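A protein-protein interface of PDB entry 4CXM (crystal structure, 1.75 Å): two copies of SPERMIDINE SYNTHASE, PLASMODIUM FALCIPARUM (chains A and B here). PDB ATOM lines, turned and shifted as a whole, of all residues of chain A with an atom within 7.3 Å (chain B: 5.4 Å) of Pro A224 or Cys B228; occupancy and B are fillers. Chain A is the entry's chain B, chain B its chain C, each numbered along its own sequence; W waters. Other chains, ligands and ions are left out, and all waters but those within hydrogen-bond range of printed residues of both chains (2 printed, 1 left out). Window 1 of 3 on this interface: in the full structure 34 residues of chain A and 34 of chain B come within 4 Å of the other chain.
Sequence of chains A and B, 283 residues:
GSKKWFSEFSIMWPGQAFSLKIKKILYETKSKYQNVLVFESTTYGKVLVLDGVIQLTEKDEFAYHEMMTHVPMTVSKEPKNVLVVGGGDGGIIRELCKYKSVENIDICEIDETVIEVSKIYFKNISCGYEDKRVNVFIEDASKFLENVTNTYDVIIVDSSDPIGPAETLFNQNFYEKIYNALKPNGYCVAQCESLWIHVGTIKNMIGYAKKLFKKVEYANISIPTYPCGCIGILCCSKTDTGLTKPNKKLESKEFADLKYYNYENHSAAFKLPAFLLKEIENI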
ATOM      1  N   PHE A  18       3.579  25.791  27.988  1.00  0.00           N
ATOM      2  CA  PHE A  18       4.713  25.069  27.480  1.00  0.00           C
ATOM      3  C   PHE A  18       5.862  26.048  27.235  1.00  0.00           C
ATOM      4  O   PHE A  18       5.646  27.157  26.732  1.00  0.00           O
ATOM      5  CB  PHE A  18       4.332  24.357  26.134  1.00  0.00           C
ATOM      6  CG  PHE A  18       5.442  23.602  25.520  1.00  0.00           C
ATOM      7  CD1 PHE A  18       5.968  22.458  26.095  1.00  0.00           C
ATOM      8  CD2 PHE A  18       5.943  24.008  24.327  1.00  0.00           C
ATOM      9  CE1 PHE A  18       6.977  21.743  25.478  1.00  0.00           C
ATOM     10  CE2 PHE A  18       7.008  23.323  23.741  1.00  0.00           C
ATOM     11  CZ  PHE A  18       7.502  22.178  24.274  1.00  0.00           C
ATOM     12  N   TYR A  44      14.735  22.230  19.941  1.00  0.00           N
ATOM     13  CA  TYR A  44      13.690  22.062  18.883  1.00  0.00           C
ATOM     14  C   TYR A  44      14.033  22.848  17.629  1.00  0.00           C
ATOM     15  O   TYR A  44      13.237  23.039  16.693  1.00  0.00           O
ATOM     16  CB  TYR A  44      12.358  22.493  19.394  1.00  0.00           C
ATOM     17  CG  TYR A  44      11.681  21.429  20.223  1.00  0.00           C
ATOM     18  CD1 TYR A  44      12.098  21.139  21.467  1.00  0.00           C
ATOM     19  CD2 TYR A  44      10.620  20.708  19.731  1.00  0.00           C
ATOM     20  CE1 TYR A  44      11.530  20.116  22.209  1.00  0.00           C
ATOM     21  CE2 TYR A  44      10.020  19.683  20.471  1.00  0.00           C
ATOM     22  CZ  TYR A  44      10.445  19.412  21.720  1.00  0.00           C
ATOM     23  OH  TYR A  44       9.921  18.419  22.489  1.00  0.00           O
ATOM     24  N   ILE A  54       3.247  29.554  19.470  1.00  0.00           N
ATOM     25  CA  ILE A  54       4.063  28.733  18.551  1.00  0.00           C
ATOM     26  C   ILE A  54       3.335  28.339  17.293  1.00  0.00           C
ATOM     27  O   ILE A  54       2.281  27.703  17.312  1.00  0.00           O
ATOM     28  CB  ILE A  54       4.632  27.478  19.272  1.00  0.00           C
ATOM     29  CG1 ILE A  54       5.484  27.901  20.509  1.00  0.00           C
ATOM     30  CG2 ILE A  54       5.556  26.670  18.359  1.00  0.00           C
ATOM     31  CD1 ILE A  54       5.820  26.796  21.515  1.00  0.00           C
ATOM     32  N   THR A  57       8.085  24.645  14.890  1.00  0.00           N
ATOM     33  CA  THR A  57       9.483  24.425  15.183  1.00  0.00           C
ATOM     34  C   THR A  57      10.109  23.589  14.069  1.00  0.00           C
ATOM     35  O   THR A  57       9.471  22.720  13.491  1.00  0.00           O
ATOM     36  CB  THR A  57       9.753  23.808  16.581  1.00  0.00           C
ATOM     37  OG1 THR A  57       9.692  22.382  16.541  1.00  0.00           O
ATOM     38  CG2 THR A  57       8.872  24.466  17.684  1.00  0.00           C
ATOM     39  N   LYS A  59      12.037  21.027  14.527  1.00  0.00           N
ATOM     40  CA  LYS A  59      12.121  19.644  14.943  1.00  0.00           C
ATOM     41  C   LYS A  59      10.854  18.836  14.551  1.00  0.00           C
ATOM     42  O   LYS A  59      10.979  17.635  14.222  1.00  0.00           O
ATOM     43  CB  LYS A  59      12.303  19.582  16.471  1.00  0.00           C
ATOM     44  CG  LYS A  59      12.232  18.187  17.112  1.00  0.00           C
ATOM     45  CD  LYS A  59      12.739  18.171  18.567  1.00  0.00           C
ATOM     46  CE  LYS A  59      12.388  16.869  19.292  1.00  0.00           C
ATOM     47  NZ  LYS A  59      13.383  15.877  18.917  1.00  0.00           N
ATOM     48  N   ASP A  60       9.676  19.439  14.657  1.00  0.00           N
ATOM     49  CA  ASP A  60       8.395  18.690  14.455  1.00  0.00           C
ATOM     50  C   ASP A  60       7.451  19.181  13.408  1.00  0.00           C
ATOM     51  O   ASP A  60       6.410  18.611  13.241  1.00  0.00           O
ATOM     52  CB  ASP A  60       7.624  18.625  15.820  1.00  0.00           C
ATOM     53  CG  ASP A  60       7.243  19.992  16.362  1.00  0.00           C
ATOM     54  OD1 ASP A  60       7.387  21.063  15.697  1.00  0.00           O
ATOM     55  OD2 ASP A  60       6.616  19.991  17.487  1.00  0.00           O
ATOM     56  N   GLU A  61       7.821  20.178  12.642  1.00  0.00           N
ATOM     57  CA  GLU A  61       6.881  20.809  11.730  1.00  0.00           C
ATOM     58  C   GLU A  61       6.400  19.836  10.638  1.00  0.00           C
ATOM     59  O   GLU A  61       5.298  19.964  10.159  1.00  0.00           O
ATOM     60  CB  GLU A  61       7.432  22.063  11.013  1.00  0.00           C
ATOM     61  CG  GLU A  61       8.769  21.802  10.296  1.00  0.00           C
ATOM     62  CD  GLU A  61       8.689  21.294   8.880  1.00  0.00           C
ATOM     63  OE1 GLU A  61       7.619  21.240   8.239  1.00  0.00           O
ATOM     64  OE2 GLU A  61       9.778  21.028   8.399  1.00  0.00           O
ATOM     65  N   ALA A  63       5.383  16.846  10.852  1.00  0.00           N
ATOM     66  CA  ALA A  63       4.205  16.068  11.243  1.00  0.00           C
ATOM     67  C   ALA A  63       2.935  16.794  10.775  1.00  0.00           C
ATOM     68  O   ALA A  63       2.050  16.240  10.159  1.00  0.00           O
ATOM     69  CB  ALA A  63       4.163  15.851  12.735  1.00  0.00           C
ATOM     70  N   ILE A 221      -3.290  14.768  14.924  1.00  0.00           N
ATOM     71  CA  ILE A 221      -1.868  14.647  14.551  1.00  0.00           C
ATOM     72  C   ILE A 221      -1.094  14.901  15.869  1.00  0.00           C
ATOM     73  O   ILE A 221      -1.478  15.878  16.567  1.00  0.00           O
ATOM     74  CB  ILE A 221      -1.491  15.805  13.609  1.00  0.00           C
ATOM     75  CG1 ILE A 221      -2.361  15.924  12.379  1.00  0.00           C
ATOM     76  CG2 ILE A 221      -0.001  15.752  13.312  1.00  0.00           C
ATOM     77  CD1 ILE A 221      -2.208  17.256  11.684  1.00  0.00           C
ATOM     78  N   SER A 222      -0.067  14.100  16.128  1.00  0.00           N
ATOM     79  CA  SER A 222       0.858  14.256  17.245  1.00  0.00           C
ATOM     80  C   SER A 222       1.879  15.265  16.901  1.00  0.00           C
ATOM     81  O   SER A 222       2.657  15.105  15.956  1.00  0.00           O
ATOM     82  CB  SER A 222       1.514  12.976  17.612  1.00  0.00           C
ATOM     83  OG  SER A 222       2.573  13.062  18.598  1.00  0.00           O
ATOM     84  N   ILE A 223       1.909  16.324  17.666  1.00  0.00           N
ATOM     85  CA  ILE A 223       2.940  17.335  17.489  1.00  0.00           C
ATOM     86  C   ILE A 223       3.273  18.044  18.789  1.00  0.00           C
ATOM     87  O   ILE A 223       2.419  18.684  19.343  1.00  0.00           O
ATOM     88  CB  ILE A 223       2.649  18.258  16.336  1.00  0.00           C
ATOM     89  CG1 ILE A 223       3.542  19.478  16.374  1.00  0.00           C
ATOM     90  CG2 ILE A 223       1.221  18.660  16.188  1.00  0.00           C
ATOM     91  CD1 ILE A 223       3.581  20.154  15.054  1.00  0.00           C
ATOM     92  N   PRO A 224       4.498  17.878  19.271  1.00  0.00           N
ATOM     93  CA  PRO A 224       4.713  18.196  20.713  1.00  0.00           C
ATOM     94  C   PRO A 224       4.696  19.674  21.082  1.00  0.00           C
ATOM     95  O   PRO A 224       4.329  20.006  22.220  1.00  0.00           O
ATOM     96  CB  PRO A 224       6.064  17.602  21.027  1.00  0.00           C
ATOM     97  CG  PRO A 224       6.775  17.497  19.667  1.00  0.00           C
ATOM     98  CD  PRO A 224       5.615  17.118  18.756  1.00  0.00           C
ATOM     99  N   THR A 225       4.823  20.537  20.093  1.00  0.00           N
ATOM    100  CA  THR A 225       4.926  21.952  20.379  1.00  0.00           C
ATOM    101  C   THR A 225       3.679  22.734  20.175  1.00  0.00           C
ATOM    102  O   THR A 225       3.733  23.973  20.144  1.00  0.00           O
ATOM    103  CB  THR A 225       6.105  22.579  19.628  1.00  0.00           C
ATOM    104  OG1 THR A 225       5.956  22.402  18.229  1.00  0.00           O
ATOM    105  CG2 THR A 225       7.422  22.002  20.067  1.00  0.00           C
ATOM    106  N   TYR A 226       2.568  22.074  19.893  1.00  0.00           N
ATOM    107  CA  TYR A 226       1.253  22.695  19.987  1.00  0.00           C
ATOM    108  C   TYR A 226       0.629  22.318  21.329  1.00  0.00           C
ATOM    109  O   TYR A 226       1.001  21.268  21.912  1.00  0.00           O
ATOM    110  CB  TYR A 226       0.353  22.255  18.858  1.00  0.00           C
ATOM    111  CG  TYR A 226       0.730  22.817  17.447  1.00  0.00           C
ATOM    112  CD1 TYR A 226       1.466  23.983  17.290  1.00  0.00           C
ATOM    113  CD2 TYR A 226       0.338  22.167  16.308  1.00  0.00           C
ATOM    114  CE1 TYR A 226       1.731  24.513  16.019  1.00  0.00           C
ATOM    115  CE2 TYR A 226       0.657  22.656  15.033  1.00  0.00           C
ATOM    116  CZ  TYR A 226       1.371  23.814  14.893  1.00  0.00           C
ATOM    117  OH  TYR A 226       1.695  24.260  13.605  1.00  0.00           O
ATOM    118  N   PRO A 227      -0.228  23.191  21.882  1.00  0.00           N
ATOM    119  CA  PRO A 227      -0.743  22.890  23.199  1.00  0.00           C
ATOM    120  C   PRO A 227      -1.413  21.535  23.317  1.00  0.00           C
ATOM    121  O   PRO A 227      -2.170  21.197  22.408  1.00  0.00           O
ATOM    122  CB  PRO A 227      -1.804  23.992  23.394  1.00  0.00           C
ATOM    123  CG  PRO A 227      -1.796  24.883  22.264  1.00  0.00           C
ATOM    124  CD  PRO A 227      -0.804  24.405  21.284  1.00  0.00           C
ATOM    125  N   CYS A 228      -1.102  20.760  24.350  1.00  0.00           N
ATOM    126  CA  CYS A 228      -1.610  19.400  24.572  1.00  0.00           C
ATOM    127  C   CYS A 228      -0.937  18.343  23.662  1.00  0.00           C
ATOM    128  O   CYS A 228      -1.289  17.187  23.734  1.00  0.00           O
ATOM    129  CB  CYS A 228      -3.110  19.301  24.487  1.00  0.00           C
ATOM    130  SG  CYS A 228      -3.909  20.201  25.913  1.00  0.00           S
ATOM    131  N   GLY A 229      -0.002  18.791  22.837  1.00  0.00           N
ATOM    132  CA  GLY A 229       0.837  17.901  22.032  1.00  0.00           C
ATOM    133  C   GLY A 229       0.113  17.319  20.858  1.00  0.00           C
ATOM    134  O   GLY A 229       0.612  16.341  20.315  1.00  0.00           O
ATOM    135  N   CYS A 230      -0.958  17.952  20.445  1.00  0.00           N
ATOM    136  CA  CYS A 230      -1.692  17.457  19.274  1.00  0.00           C
ATOM    137  C   CYS A 230      -2.542  18.544  18.639  1.00  0.00           C
ATOM    138  O   CYS A 230      -2.865  19.541  19.250  1.00  0.00           O
ATOM    139  CB  CYS A 230      -2.498  16.223  19.584  1.00  0.00           C
ATOM    140  SG  CYS A 230      -3.822  16.435  20.782  1.00  0.00           S
ATOM    141  N   GLN B  16      12.905  21.852  27.377  1.00  0.00           N
ATOM    142  CA  GLN B  16      11.471  22.015  27.374  1.00  0.00           C
ATOM    143  C   GLN B  16      10.889  21.846  28.741  1.00  0.00           C
ATOM    144  O   GLN B  16      11.454  21.108  29.605  1.00  0.00           O
ATOM    145  CB  GLN B  16      10.808  21.013  26.369  1.00  0.00           C
ATOM    146  CG  GLN B  16      10.888  19.568  26.882  1.00  0.00           C
ATOM    147  CD  GLN B  16      10.406  18.559  25.877  1.00  0.00           C
ATOM    148  OE1 GLN B  16      11.116  18.230  24.923  1.00  0.00           O
ATOM    149  NE2 GLN B  16       9.192  18.040  26.082  1.00  0.00           N
ATOM    150  N   SER B 194       8.651   8.735  25.154  1.00  0.00           N
ATOM    151  CA  SER B 194       8.018   9.512  24.103  1.00  0.00           C
ATOM    152  C   SER B 194       8.837   9.355  22.814  1.00  0.00           C
ATOM    153  O   SER B 194      10.011   9.603  22.798  1.00  0.00           O
ATOM    154  CB  SER B 194       7.993  10.970  24.392  1.00  0.00           C
ATOM    155  OG  SER B 194       7.343  11.615  23.323  1.00  0.00           O
ATOM    156  N   TRP B 196       9.117  11.433  20.471  1.00  0.00           N
ATOM    157  CA  TRP B 196       9.577  12.708  20.031  1.00  0.00           C
ATOM    158  C   TRP B 196      10.920  13.029  20.628  1.00  0.00           C
ATOM    159  O   TRP B 196      11.666  13.682  19.933  1.00  0.00           O
ATOM    160  CB  TRP B 196       8.567  13.756  20.265  1.00  0.00           C
ATOM    161  CG  TRP B 196       7.444  13.797  19.359  1.00  0.00           C
ATOM    162  CD1 TRP B 196       6.208  13.370  19.554  1.00  0.00           C
ATOM    163  CD2 TRP B 196       7.527  14.207  17.992  1.00  0.00           C
ATOM    164  NE1 TRP B 196       5.480  13.484  18.399  1.00  0.00           N
ATOM    165  CE2 TRP B 196       6.278  14.047  17.442  1.00  0.00           C
ATOM    166  CE3 TRP B 196       8.579  14.698  17.188  1.00  0.00           C
ATOM    167  CZ2 TRP B 196       5.980  14.404  16.095  1.00  0.00           C
ATOM    168  CZ3 TRP B 196       8.299  15.048  15.822  1.00  0.00           C
ATOM    169  CH2 TRP B 196       7.004  14.888  15.305  1.00  0.00           C
ATOM    170  N   ILE B 197      11.295  12.415  21.707  1.00  0.00           N
ATOM    171  CA  ILE B 197      12.567  12.786  22.382  1.00  0.00           C
ATOM    172  C   ILE B 197      13.356  11.626  22.984  1.00  0.00           C
ATOM    173  O   ILE B 197      14.498  11.819  23.453  1.00  0.00           O
ATOM    174  CB  ILE B 197      12.294  13.844  23.499  1.00  0.00           C
ATOM    175  CG1 ILE B 197      11.141  13.344  24.354  1.00  0.00           C
ATOM    176  CG2 ILE B 197      12.023  15.255  22.893  1.00  0.00           C
ATOM    177  CD1 ILE B 197      10.980  14.236  25.630  1.00  0.00           C
ATOM    178  N   TYR B 226       1.996  14.200  29.775  1.00  0.00           N
ATOM    179  CA  TYR B 226       3.349  13.627  29.718  1.00  0.00           C
ATOM    180  C   TYR B 226       4.138  14.350  28.571  1.00  0.00           C
ATOM    181  O   TYR B 226       3.531  14.974  27.702  1.00  0.00           O
ATOM    182  CB  TYR B 226       3.355  12.124  29.439  1.00  0.00           C
ATOM    183  CG  TYR B 226       2.805  11.201  30.483  1.00  0.00           C
ATOM    184  CD1 TYR B 226       2.989  11.455  31.858  1.00  0.00           C
ATOM    185  CD2 TYR B 226       2.167  10.009  30.137  1.00  0.00           C
ATOM    186  CE1 TYR B 226       2.615  10.545  32.799  1.00  0.00           C
ATOM    187  CE2 TYR B 226       1.729   9.109  31.117  1.00  0.00           C
ATOM    188  CZ  TYR B 226       1.915   9.413  32.472  1.00  0.00           C
ATOM    189  OH  TYR B 226       1.501   8.456  33.363  1.00  0.00           O
ATOM    190  N   PRO B 227       5.447  14.509  28.772  1.00  0.00           N
ATOM    191  CA  PRO B 227       6.319  15.351  27.947  1.00  0.00           C
ATOM    192  C   PRO B 227       6.121  14.982  26.455  1.00  0.00           C
ATOM    193  O   PRO B 227       6.080  13.764  26.162  1.00  0.00           O
ATOM    194  CB  PRO B 227       7.698  15.000  28.431  1.00  0.00           C
ATOM    195  CG  PRO B 227       7.521  14.390  29.831  1.00  0.00           C
ATOM    196  CD  PRO B 227       6.168  13.798  29.841  1.00  0.00           C
ATOM    197  N   CYS B 228       5.880  15.993  25.626  1.00  0.00           N
ATOM    198  CA  CYS B 228       5.611  15.841  24.164  1.00  0.00           C
ATOM    199  C   CYS B 228       4.220  15.393  23.875  1.00  0.00           C
ATOM    200  O   CYS B 228       3.843  15.293  22.685  1.00  0.00           O
ATOM    201  CB  CYS B 228       6.657  14.955  23.545  1.00  0.00           C
ATOM    202  SG  CYS B 228       8.324  15.690  23.598  1.00  0.00           S
ATOM    203  N   GLY B 229       3.379  15.190  24.958  1.00  0.00           N
ATOM    204  CA  GLY B 229       1.991  14.903  24.737  1.00  0.00           C
ATOM    205  C   GLY B 229       1.680  13.483  24.331  1.00  0.00           C
ATOM    206  O   GLY B 229       0.536  13.202  23.907  1.00  0.00           O
ATOM    207  N   CYS B 230       2.646  12.593  24.507  1.00  0.00           N
ATOM    208  CA  CYS B 230       2.492  11.179  24.166  1.00  0.00           C
ATOM    209  C   CYS B 230       3.428  10.304  24.929  1.00  0.00           C
ATOM    210  O   CYS B 230       4.468  10.740  25.470  1.00  0.00           O
ATOM    211  CB  CYS B 230       2.599  10.922  22.676  1.00  0.00           C
ATOM    212  SG  CYS B 230       4.225  11.229  21.947  1.00  0.00           S
HETATM  213  O   HOH W   1      12.008  14.132  16.647  1.00  0.00           O
HETATM  214  O   HOH W   2      -1.361  14.649  22.674  1.00  0.00           O
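The side-chain amino group (NZ) of Lys A59 is in hydrogen-bond range of the backbone carbonyl oxygen (O) of Trp B196 (3.0 Å). The side-chain hydroxyl (OG) of Ser A222 lies within hydrogen-bond range of the indole nitrogen (NE1) of Trp B196 (2.9 Å). The side-chain hydroxyl (OH) of Tyr A44 is in hydrogen-bond range of the side-chain amide oxygen (OE1) of Gln B16 (2.7 Å). The side-chain hydroxyl (OH) of Tyr A44 is in hydrogen-bond range of the side-chain sulfur (SG) of Cys B228, at 3.4 Å.
Water W2 lies within hydrogen-bond range of O of Gly B229 (2.7 Å), O of Cys A228 (2.8 Å) and SG of Cys A230 (3.6 Å). Water W1 lies within hydrogen-bond range of NZ of Lys A59 (3.2 Å) and O of Trp B196 (3.3 Å).
N of Trp B196 sits close to OG of Ser B194. N of Lys A59 is in hydrogen-bond range of O of Tyr A44. The side-chain sulfur of Cys B228 sits at hydrogen-bond distance from the side-chain amide nitrogen of Gln B16 (3.5 Å). OG1 of Thr A57 lies close to N of Lys A59, at 3.4 Å. OD1 of Asp A60 lies within hydrogen-bond range of OG1 of Thr A57 (2.8 Å). OD2 of Asp A60 lies within hydrogen-bond range of OG1 of Thr A225 (2.6 Å).
Tyr A44 touches Ile B197 (OH to CG2, 3.8 Å). Lys A59 touches Ile B197. CZ3 of Trp B196 touches CB of Asp A60, at 3.6 Å. Trp B196 touches Ala A63. Pro A224 touches Trp B196. CB of Pro A224 touches O of Cys B228 (3.6 Å).
Hydrophobic or aromatic side chains of chain A that line the printed part of chain B: Tyr A44, Ala A63 and Pro A224. Of the 9 printed residues of chain B, 4 touch a printed residue of chain A. Hydrophobic or aromatic side chains of chain B within 4 Å of the printed part of chain A: Trp B196 and Ile B197. Among the printed residues, 10 pairs touch across the chains. Among the printed residues, no Asp or Glu carboxylate lies within 4 Å of a Lys or Arg side-chain nitrogen of the other chain.
5 positions are printed for both chains. Of the 10 pairs that touch across the chains among the printed residues, none has its exchanged pair printed and touching as well.
Pro A224 touches two residues of chain B. Cys B228 touches just these residues of chain A: Tyr A44 and Pro A224. Of the printed residues of chain A, Gln B16 touches Tyr A44. Printed residues of chain A within 4 Å of Trp B196: Lys A59 (3.0 Å), Asp A60 (3.6 Å), Ala A63 (3.95 Å), Ser A222 (2.9 Å) and Pro A224 (3.4 Å). Of the printed residues of chain B, Ala A63 touches Trp B196. Of the printed residues of chain A, Ile B197 touches Tyr A44 and Lys A59. Of the printed residues of chain B, Ser A222 touches Trp B196. Thr A225 touches none of the printed residues of chain B. Ile A223 touches none of the printed residues of chain B. The nearest residue of chain B that does not touch Pro A224 is Gly B229 (5.3 Å). The nearest residue of chain A that does not touch Cys B228 is Gly A229 (4.03 Å). The nearest printed residue of chain B that does not touch Asp A60 is Cys B228 (7.5 Å).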
